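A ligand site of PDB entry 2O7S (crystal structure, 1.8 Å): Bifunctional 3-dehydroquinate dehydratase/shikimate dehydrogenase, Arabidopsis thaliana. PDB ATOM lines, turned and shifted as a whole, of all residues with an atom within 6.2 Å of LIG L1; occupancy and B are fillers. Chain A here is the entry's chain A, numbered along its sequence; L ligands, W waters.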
ATOM      1  N   ILE A 239      10.544   6.316  33.684  1.00  0.00           N
ATOM      2  CA  ILE A 239       9.262   5.698  33.420  1.00  0.00           C
ATOM      3  C   ILE A 239       8.510   5.523  34.749  1.00  0.00           C
ATOM      4  O   ILE A 239       8.966   4.807  35.648  1.00  0.00           O
ATOM      5  CB  ILE A 239       9.436   4.314  32.725  1.00  0.00           C
ATOM      6  CG1 ILE A 239       8.097   3.569  32.702  1.00  0.00           C
ATOM      7  CG2 ILE A 239      10.525   3.487  33.417  1.00  0.00           C
ATOM      8  CD1 ILE A 239       7.007   4.255  31.876  1.00  0.00           C
ATOM      9  N   HIS A 246       9.205  -4.276  34.556  1.00  0.00           N
ATOM     10  CA  HIS A 246       9.188  -4.894  33.234  1.00  0.00           C
ATOM     11  C   HIS A 246       9.556  -3.903  32.131  1.00  0.00           C
ATOM     12  O   HIS A 246       9.821  -4.302  31.008  1.00  0.00           O
ATOM     13  CB  HIS A 246       7.802  -5.420  32.927  1.00  0.00           C
ATOM     14  CG  HIS A 246       6.769  -4.335  32.869  1.00  0.00           C
ATOM     15  ND1 HIS A 246       6.192  -3.797  33.993  1.00  0.00           N
ATOM     16  CD2 HIS A 246       6.288  -3.623  31.824  1.00  0.00           C
ATOM     17  CE1 HIS A 246       5.399  -2.801  33.647  1.00  0.00           C
ATOM     18  NE2 HIS A 246       5.439  -2.672  32.332  1.00  0.00           N
ATOM     19  N   SER A 247       9.541  -2.614  32.458  1.00  0.00           N
ATOM     20  CA  SER A 247       9.791  -1.588  31.430  1.00  0.00           C
ATOM     21  C   SER A 247      11.149  -1.594  30.746  1.00  0.00           C
ATOM     22  O   SER A 247      12.190  -1.675  31.389  1.00  0.00           O
ATOM     23  CB  SER A 247       9.554  -0.195  31.998  1.00  0.00           C
ATOM     24  OG  SER A 247       9.908   0.791  31.031  1.00  0.00           O
ATOM     25  N   LYS A 248      11.117  -1.458  29.414  1.00  0.00           N
ATOM     26  CA  LYS A 248      12.334  -1.390  28.618  1.00  0.00           C
ATOM     27  C   LYS A 248      12.611   0.042  28.167  1.00  0.00           C
ATOM     28  O   LYS A 248      13.496   0.267  27.346  1.00  0.00           O
ATOM     29  CB  LYS A 248      12.211  -2.327  27.399  1.00  0.00           C
ATOM     30  CG  LYS A 248      12.249  -3.795  27.792  1.00  0.00           C
ATOM     31  CD  LYS A 248      12.266  -4.713  26.597  1.00  0.00           C
ATOM     32  CE  LYS A 248      12.441  -6.164  27.048  1.00  0.00           C
ATOM     33  NZ  LYS A 248      12.298  -7.117  25.912  1.00  0.00           N
ATOM     34  N   SER A 249      11.850   1.011  28.693  1.00  0.00           N
ATOM     35  CA  SER A 249      12.088   2.413  28.324  1.00  0.00           C
ATOM     36  C   SER A 249      13.514   2.825  28.678  1.00  0.00           C
ATOM     37  O   SER A 249      14.174   3.534  27.911  1.00  0.00           O
ATOM     38  CB  SER A 249      11.064   3.346  28.991  1.00  0.00           C
ATOM     39  OG  SER A 249       9.852   3.383  28.241  1.00  0.00           O
ATOM     40  N   PRO A 250      14.018   2.391  29.843  1.00  0.00           N
ATOM     41  CA  PRO A 250      15.385   2.780  30.186  1.00  0.00           C
ATOM     42  C   PRO A 250      16.411   2.209  29.194  1.00  0.00           C
ATOM     43  O   PRO A 250      17.468   2.808  28.964  1.00  0.00           O
ATOM     44  CB  PRO A 250      15.562   2.224  31.595  1.00  0.00           C
ATOM     45  CG  PRO A 250      14.158   2.294  32.160  1.00  0.00           C
ATOM     46  CD  PRO A 250      13.333   1.783  31.006  1.00  0.00           C
ATOM     47  N   TYR A 266      18.058   7.992  31.955  1.00  0.00           N
ATOM     48  CA  TYR A 266      16.676   7.531  32.123  1.00  0.00           C
ATOM     49  C   TYR A 266      16.592   6.325  33.087  1.00  0.00           C
ATOM     50  O   TYR A 266      17.285   5.327  32.879  1.00  0.00           O
ATOM     51  CB  TYR A 266      16.131   7.173  30.738  1.00  0.00           C
ATOM     52  CG  TYR A 266      14.634   7.019  30.640  1.00  0.00           C
ATOM     53  CD1 TYR A 266      14.001   5.881  31.135  1.00  0.00           C
ATOM     54  CD2 TYR A 266      13.850   8.001  30.003  1.00  0.00           C
ATOM     55  CE1 TYR A 266      12.629   5.712  31.003  1.00  0.00           C
ATOM     56  CE2 TYR A 266      12.478   7.832  29.871  1.00  0.00           C
ATOM     57  CZ  TYR A 266      11.874   6.689  30.373  1.00  0.00           C
ATOM     58  OH  TYR A 266      10.527   6.485  30.231  1.00  0.00           O
ATOM     59  N   SER A 290       7.848   9.408  31.398  1.00  0.00           N
ATOM     60  CA  SER A 290       6.966   8.605  30.582  1.00  0.00           C
ATOM     61  C   SER A 290       6.037   8.020  31.660  1.00  0.00           C
ATOM     62  O   SER A 290       6.472   7.797  32.785  1.00  0.00           O
ATOM     63  CB  SER A 290       7.740   7.478  29.880  1.00  0.00           C
ATOM     64  OG  SER A 290       8.719   8.009  29.010  1.00  0.00           O
ATOM     65  N   CYS A 291       4.772   7.805  31.311  1.00  0.00           N
ATOM     66  CA  CYS A 291       3.815   7.257  32.275  1.00  0.00           C
ATOM     67  C   CYS A 291       3.100   6.035  31.753  1.00  0.00           C
ATOM     68  O   CYS A 291       2.512   6.062  30.676  1.00  0.00           O
ATOM     69  CB  CYS A 291       2.762   8.311  32.634  1.00  0.00           C
ATOM     70  SG  CYS A 291       3.413   9.792  33.384  1.00  0.00           S
ATOM     71  N   THR A 292       3.125   4.957  32.528  1.00  0.00           N
ATOM     72  CA  THR A 292       2.462   3.743  32.137  1.00  0.00           C
ATOM     73  C   THR A 292       1.503   3.315  33.240  1.00  0.00           C
ATOM     74  O   THR A 292       1.302   4.045  34.212  1.00  0.00           O
ATOM     75  CB  THR A 292       3.478   2.599  31.842  1.00  0.00           C
ATOM     76  OG1 THR A 292       2.793   1.496  31.234  1.00  0.00           O
ATOM     77  CG2 THR A 292       4.161   2.128  33.118  1.00  0.00           C
ATOM     78  N   ILE A 293       0.903   2.142  33.074  1.00  0.00           N
ATOM     79  CA  ILE A 293      -0.045   1.595  34.032  1.00  0.00           C
ATOM     80  C   ILE A 293       0.408   1.862  35.467  1.00  0.00           C
ATOM     81  O   ILE A 293       1.552   1.582  35.830  1.00  0.00           O
ATOM     82  CB  ILE A 293      -0.200   0.066  33.791  1.00  0.00           C
ATOM     83  CG1 ILE A 293      -1.170  -0.537  34.790  1.00  0.00           C
ATOM     84  CG2 ILE A 293       1.164  -0.604  33.862  1.00  0.00           C
ATOM     85  CD1 ILE A 293      -1.462  -2.002  34.539  1.00  0.00           C
ATOM     86  N   LYS A 296      -1.665   6.850  33.836  1.00  0.00           N
ATOM     87  CA  LYS A 296      -1.940   7.678  32.662  1.00  0.00           C
ATOM     88  C   LYS A 296      -3.047   8.713  32.882  1.00  0.00           C
ATOM     89  O   LYS A 296      -2.974   9.828  32.370  1.00  0.00           O
ATOM     90  CB  LYS A 296      -2.285   6.798  31.448  1.00  0.00           C
ATOM     91  CG  LYS A 296      -1.097   5.989  30.907  1.00  0.00           C
ATOM     92  CD  LYS A 296      -1.501   5.189  29.660  1.00  0.00           C
ATOM     93  CE  LYS A 296      -0.391   4.250  29.199  1.00  0.00           C
ATOM     94  NZ  LYS A 296       0.836   4.949  28.713  1.00  0.00           N
ATOM     95  N   ASN A 317       0.709  10.101  28.654  1.00  0.00           N
ATOM     96  CA  ASN A 317       1.800   9.149  28.840  1.00  0.00           C
ATOM     97  C   ASN A 317       3.167   9.840  28.771  1.00  0.00           C
ATOM     98  O   ASN A 317       4.194   9.182  28.916  1.00  0.00           O
ATOM     99  CB  ASN A 317       1.747   8.030  27.796  1.00  0.00           C
ATOM    100  CG  ASN A 317       2.341   8.437  26.463  1.00  0.00           C
ATOM    101  OD1 ASN A 317       2.898   7.603  25.739  1.00  0.00           O
ATOM    102  ND2 ASN A 317       2.222   9.715  26.124  1.00  0.00           N
ATOM    103  N   THR A 318       3.171  11.151  28.555  1.00  0.00           N
ATOM    104  CA  THR A 318       4.425  11.901  28.476  1.00  0.00           C
ATOM    105  C   THR A 318       4.325  13.248  29.202  1.00  0.00           C
ATOM    106  O   THR A 318       3.450  14.073  28.896  1.00  0.00           O
ATOM    107  CB  THR A 318       4.847  12.173  27.001  1.00  0.00           C
ATOM    108  OG1 THR A 318       4.570  11.014  26.203  1.00  0.00           O
ATOM    109  CG2 THR A 318       6.325  12.479  26.921  1.00  0.00           C
ATOM    110  N   THR A 333       1.595  10.036  23.277  1.00  0.00           N
ATOM    111  CA  THR A 333       2.183   9.408  22.099  1.00  0.00           C
ATOM    112  C   THR A 333       1.652   7.995  21.861  1.00  0.00           C
ATOM    113  O   THR A 333       2.025   7.341  20.888  1.00  0.00           O
ATOM    114  CB  THR A 333       3.741   9.360  22.205  1.00  0.00           C
ATOM    115  OG1 THR A 333       4.125   8.535  23.305  1.00  0.00           O
ATOM    116  CG2 THR A 333       4.305  10.760  22.414  1.00  0.00           C
ATOM    117  N   ASP A 334       0.776   7.526  22.748  1.00  0.00           N
ATOM    118  CA  ASP A 334       0.178   6.200  22.609  1.00  0.00           C
ATOM    119  C   ASP A 334      -0.751   6.087  21.404  1.00  0.00           C
ATOM    120  O   ASP A 334      -0.755   5.076  20.702  1.00  0.00           O
ATOM    121  CB  ASP A 334      -0.617   5.813  23.868  1.00  0.00           C
ATOM    122  CG  ASP A 334       0.262   5.405  25.039  1.00  0.00           C
ATOM    123  OD1 ASP A 334       1.261   4.675  24.827  1.00  0.00           O
ATOM    124  OD2 ASP A 334      -0.044   5.785  26.186  1.00  0.00           O
ATOM    125  N   TYR A 461       3.838  -5.548  25.622  1.00  0.00           N
ATOM    126  CA  TYR A 461       5.054  -5.838  24.874  1.00  0.00           C
ATOM    127  C   TYR A 461       6.081  -6.648  25.668  1.00  0.00           C
ATOM    128  O   TYR A 461       7.177  -6.926  25.183  1.00  0.00           O
ATOM    129  CB  TYR A 461       5.697  -4.543  24.334  1.00  0.00           C
ATOM    130  CG  TYR A 461       6.379  -3.683  25.372  1.00  0.00           C
ATOM    131  CD1 TYR A 461       5.645  -2.897  26.259  1.00  0.00           C
ATOM    132  CD2 TYR A 461       7.774  -3.672  25.484  1.00  0.00           C
ATOM    133  CE1 TYR A 461       6.272  -2.119  27.233  1.00  0.00           C
ATOM    134  CE2 TYR A 461       8.414  -2.901  26.439  1.00  0.00           C
ATOM    135  CZ  TYR A 461       7.666  -2.139  27.313  1.00  0.00           C
ATOM    136  OH  TYR A 461       8.313  -1.397  28.268  1.00  0.00           O
ATOM    137  N   MET A 485       4.155  -0.888  18.691  1.00  0.00           N
ATOM    138  CA  MET A 485       3.567   0.289  19.306  1.00  0.00           C
ATOM    139  C   MET A 485       4.569   0.951  20.253  1.00  0.00           C
ATOM    140  O   MET A 485       4.636   2.179  20.355  1.00  0.00           O
ATOM    141  CB  MET A 485       2.313  -0.104  20.098  1.00  0.00           C
ATOM    142  CG  MET A 485       1.754   1.035  20.931  1.00  0.00           C
ATOM    143  SD  MET A 485       0.400   0.525  22.034  1.00  0.00           S
ATOM    144  CE  MET A 485      -0.182   2.143  22.601  1.00  0.00           C
ATOM    145  N   PHE A 486       5.354   0.133  20.953  1.00  0.00           N
ATOM    146  CA  PHE A 486       6.344   0.629  21.901  1.00  0.00           C
ATOM    147  C   PHE A 486       7.441   1.477  21.266  1.00  0.00           C
ATOM    148  O   PHE A 486       7.758   2.557  21.762  1.00  0.00           O
ATOM    149  CB  PHE A 486       6.999  -0.533  22.653  1.00  0.00           C
ATOM    150  CG  PHE A 486       8.009  -0.095  23.675  1.00  0.00           C
ATOM    151  CD1 PHE A 486       7.589   0.516  24.852  1.00  0.00           C
ATOM    152  CD2 PHE A 486       9.367  -0.261  23.457  1.00  0.00           C
ATOM    153  CE1 PHE A 486       8.528   0.971  25.798  1.00  0.00           C
ATOM    154  CE2 PHE A 486      10.313   0.175  24.389  1.00  0.00           C
ATOM    155  CZ  PHE A 486       9.882   0.794  25.572  1.00  0.00           C
ATOM    156  N   GLN A 489       5.827   4.942  19.981  1.00  0.00           N
ATOM    157  CA  GLN A 489       5.519   5.936  20.987  1.00  0.00           C
ATOM    158  C   GLN A 489       6.796   6.424  21.658  1.00  0.00           C
ATOM    159  O   GLN A 489       6.849   7.561  22.146  1.00  0.00           O
ATOM    160  CB  GLN A 489       4.549   5.363  22.040  1.00  0.00           C
ATOM    161  CG  GLN A 489       5.108   4.250  22.910  1.00  0.00           C
ATOM    162  CD  GLN A 489       5.947   4.764  24.068  1.00  0.00           C
ATOM    163  OE1 GLN A 489       5.631   5.793  24.671  1.00  0.00           O
ATOM    164  NE2 GLN A 489       7.003   4.037  24.399  1.00  0.00           N
ATOM    165  N   GLN A 493       8.536  10.340  22.101  1.00  0.00           N
ATOM    166  CA  GLN A 493       8.836  10.893  23.420  1.00  0.00           C
ATOM    167  C   GLN A 493      10.254  11.471  23.438  1.00  0.00           C
ATOM    168  O   GLN A 493      10.520  12.455  24.133  1.00  0.00           O
ATOM    169  CB  GLN A 493       8.709   9.819  24.522  1.00  0.00           C
ATOM    170  CG  GLN A 493       7.291   9.329  24.818  1.00  0.00           C
ATOM    171  CD  GLN A 493       7.206   8.526  26.111  1.00  0.00           C
ATOM    172  OE1 GLN A 493       8.121   7.781  26.454  1.00  0.00           O
ATOM    173  NE2 GLN A 493       6.087   8.673  26.830  1.00  0.00           N
HETATM  174  C1  LIG L   1       4.723   1.752  28.404  1.00  0.00           C
HETATM  175  C2  LIG L   1       3.616   2.544  27.749  1.00  0.00           C
HETATM  176  O1  LIG L   1       2.583   2.766  28.723  1.00  0.00           O
HETATM  177  C3  LIG L   1       4.082   3.915  27.174  1.00  0.00           C
HETATM  178  O2  LIG L   1       2.952   4.777  27.009  1.00  0.00           O
HETATM  179  C4  LIG L   1       5.134   4.568  28.105  1.00  0.00           C
HETATM  180  C5  LIG L   1       5.933   2.223  28.631  1.00  0.00           C
HETATM  181  C6  LIG L   1       6.360   3.643  28.269  1.00  0.00           C
HETATM  182  C7  LIG L   1       6.925   1.345  29.279  1.00  0.00           C
HETATM  183  O3  LIG L   1       8.155   1.810  29.518  1.00  0.00           O
HETATM  184  O4  LIG L   1       6.628   0.197  29.597  1.00  0.00           O
HETATM  185  O5  LIG L   1       5.561   5.827  27.565  1.00  0.00           O
HETATM  186  P1  LG2 L   2      -4.754   1.091  32.888  1.00  0.00           P
HETATM  187  O1  LG2 L   2      -4.212   0.673  34.203  1.00  0.00           O
HETATM  188  O2  LG2 L   2      -4.425   2.413  32.303  1.00  0.00           O
HETATM  189  O3  LG2 L   2      -5.319  -0.042  31.869  1.00  0.00           O
HETATM  190  C1  LG2 L   2      -5.453  -1.305  32.545  1.00  0.00           C
HETATM  191  C2  LG2 L   2      -6.601  -2.125  31.973  1.00  0.00           C
HETATM  192  O4  LG2 L   2      -6.325  -3.453  32.401  1.00  0.00           O
HETATM  193  C3  LG2 L   2      -8.087  -2.027  32.270  1.00  0.00           C
HETATM  194  O5  LG2 L   2      -8.964  -2.038  31.129  1.00  0.00           O
HETATM  195  C4  LG2 L   2      -8.228  -2.710  33.651  1.00  0.00           C
HETATM  196  O6  LG2 L   2      -9.465  -3.457  33.779  1.00  0.00           O
HETATM  197  C5  LG2 L   2      -6.961  -3.623  33.629  1.00  0.00           C
HETATM  198  N1  LG2 L   2      -6.983  -5.042  34.016  1.00  0.00           N
HETATM  199  C6  LG2 L   2      -6.150  -5.640  34.979  1.00  0.00           C
HETATM  200  N2  LG2 L   2      -6.433  -6.966  35.077  1.00  0.00           N
HETATM  201  C7  LG2 L   2      -7.435  -7.170  34.176  1.00  0.00           C
HETATM  202  C8  LG2 L   2      -8.070  -8.379  33.895  1.00  0.00           C
HETATM  203  N3  LG2 L   2      -7.709  -9.478  34.552  1.00  0.00           N
HETATM  204  N4  LG2 L   2      -9.093  -8.433  32.933  1.00  0.00           N
HETATM  205  C9  LG2 L   2      -9.437  -7.217  32.266  1.00  0.00           C
HETATM  206  N5  LG2 L   2      -8.757  -6.020  32.580  1.00  0.00           N
HETATM  207  C10 LG2 L   2      -7.757  -6.094  33.557  1.00  0.00           C
HETATM  208  O7  LG2 L   2      -3.292   0.572  32.416  1.00  0.00           O
HETATM  209  P2  LG2 L   2      -2.675   1.119  30.953  1.00  0.00           P
HETATM  210  O8  LG2 L   2      -1.934   2.381  31.192  1.00  0.00           O
HETATM  211  O9  LG2 L   2      -3.773   1.377  29.956  1.00  0.00           O
HETATM  212  O10 LG2 L   2      -1.637   0.025  30.353  1.00  0.00           O
HETATM  213  C11 LG2 L   2      -2.290  -1.250  30.078  1.00  0.00           C
HETATM  214  C12 LG2 L   2      -1.332  -2.310  29.473  1.00  0.00           C
HETATM  215  O11 LG2 L   2      -1.015  -2.111  28.053  1.00  0.00           O
HETATM  216  C13 LG2 L   2       0.036  -2.437  30.213  1.00  0.00           C
HETATM  217  O12 LG2 L   2       0.306  -3.854  30.377  1.00  0.00           O
HETATM  218  C14 LG2 L   2       1.033  -1.820  29.324  1.00  0.00           C
HETATM  219  O13 LG2 L   2       2.285  -2.461  29.375  1.00  0.00           O
HETATM  220  C15 LG2 L   2       0.412  -1.886  27.917  1.00  0.00           C
HETATM  221  N6  LG2 L   2       0.757  -0.711  27.085  1.00  0.00           N
HETATM  222  C16 LG2 L   2       1.758  -0.929  26.117  1.00  0.00           C
HETATM  223  C17 LG2 L   2       2.082   0.201  25.313  1.00  0.00           C
HETATM  224  C18 LG2 L   2       3.125   0.064  24.267  1.00  0.00           C
HETATM  225  O14 LG2 L   2       3.431   1.016  23.549  1.00  0.00           O
HETATM  226  N7  LG2 L   2       3.749  -1.122  24.093  1.00  0.00           N
HETATM  227  C19 LG2 L   2       1.413   1.470  25.481  1.00  0.00           C
HETATM  228  C20 LG2 L   2       0.431   1.621  26.457  1.00  0.00           C
HETATM  229  C21 LG2 L   2       0.076   0.535  27.285  1.00  0.00           C
HETATM  230  P3  LG2 L   2     -10.544  -2.589  34.610  1.00  0.00           P
HETATM  231  O15 LG2 L   2     -10.864  -1.316  33.866  1.00  0.00           O
HETATM  232  O16 LG2 L   2     -11.767  -3.343  34.741  1.00  0.00           O
HETATM  233  O17 LG2 L   2     -10.008  -2.253  35.933  1.00  0.00           O
HETATM  234  O   HOH W   1       4.305  -0.746  30.598  1.00  0.00           O
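OG of Ser 247 lies within hydrogen-bond range of O3 of LIG L1, at 2.5 Å.
The side-chain hydroxyl (OG) of Ser 249 is in hydrogen-bond range of an oxygen (O3) of LIG L1 (2.6 Å).
An oxygen (O4) of LIG L1 is in hydrogen-bond range of the side-chain hydroxyl (OH) of Tyr 461 (2.7 Å).
NZ of Lys 296 sits at hydrogen-bond distance from O2 of LIG L1, at 2.7 Å.
OD1 of Asp 334 sits at hydrogen-bond distance from O2 of LIG L1 (2.8 Å).
OG1 of Thr 292 lies within hydrogen-bond range of O1 of LIG L1.
O5 of LIG L1 sits at hydrogen-bond distance from OE1 of Gln 489 (2.9 Å).
The side-chain amide nitrogen of Gln 493 sits at hydrogen-bond distance from an oxygen (O5) of LIG L1 (3.0 Å).
OD1 of Asn 317 lies within hydrogen-bond range of O2 of LIG L1, at 3.1 Å.
The backbone NH (N) of Phe 486 lies within hydrogen-bond range of an oxygen (O14) of LG2 L2.
The backbone NH of Ile 293 lies within hydrogen-bond range of an oxygen (O8) of LG2 L2 (3.4 Å).
The side-chain amino group (NZ) of Lys 296 lies within salt-bridge range of the side-chain carboxylate (OD2) of Asp 334 (2.8 Å).
O of Cys 291 sits at hydrogen-bond distance from NZ of Lys 296, at 2.8 Å.
OD1 of Asn 317 lies close to OD1 of Asp 334, at 3.5 Å.
NE2 of Gln 489 sits at hydrogen-bond distance from O of Phe 486 (3.1 Å).
The backbone NH of Cys 291 sits at hydrogen-bond distance from the backbone carbonyl oxygen of Asn 317.
The side-chain hydroxyl (OG1) of Thr 333 is in hydrogen-bond range of the side-chain amide oxygen (OD1) of Asn 317 (2.9 Å).
OG1 of Thr 318 sits at hydrogen-bond distance from ND2 of Asn 317 (2.7 Å).
The backbone NH (N) of Ile 239 sits close to the side-chain hydroxyl (OH) of Tyr 266 (3.5 Å).
Residues that only touch LIG L1: Ser 290 (3.6 Å), Ile 239 (3.6 Å), Phe 486 (3.8 Å) and Cys 291 (3.8 Å).
13 residues have an atom within 4 Å of LIG L1: Ile 239, Ser 247, Ser 249, Ser 290, Cys 291, Thr 292, Lys 296, Asn 317, Asp 334, Tyr 461, Phe 486, Gln 489 and Gln 493.
The nearest printed residue that does not touch LIG L1 is His 246 (4.1 Å).
Water W1 lies within hydrogen-bond range of O4 of LIG L1, OG1 of Thr 292, NE2 of His 246 and O13 of LG2 L2.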
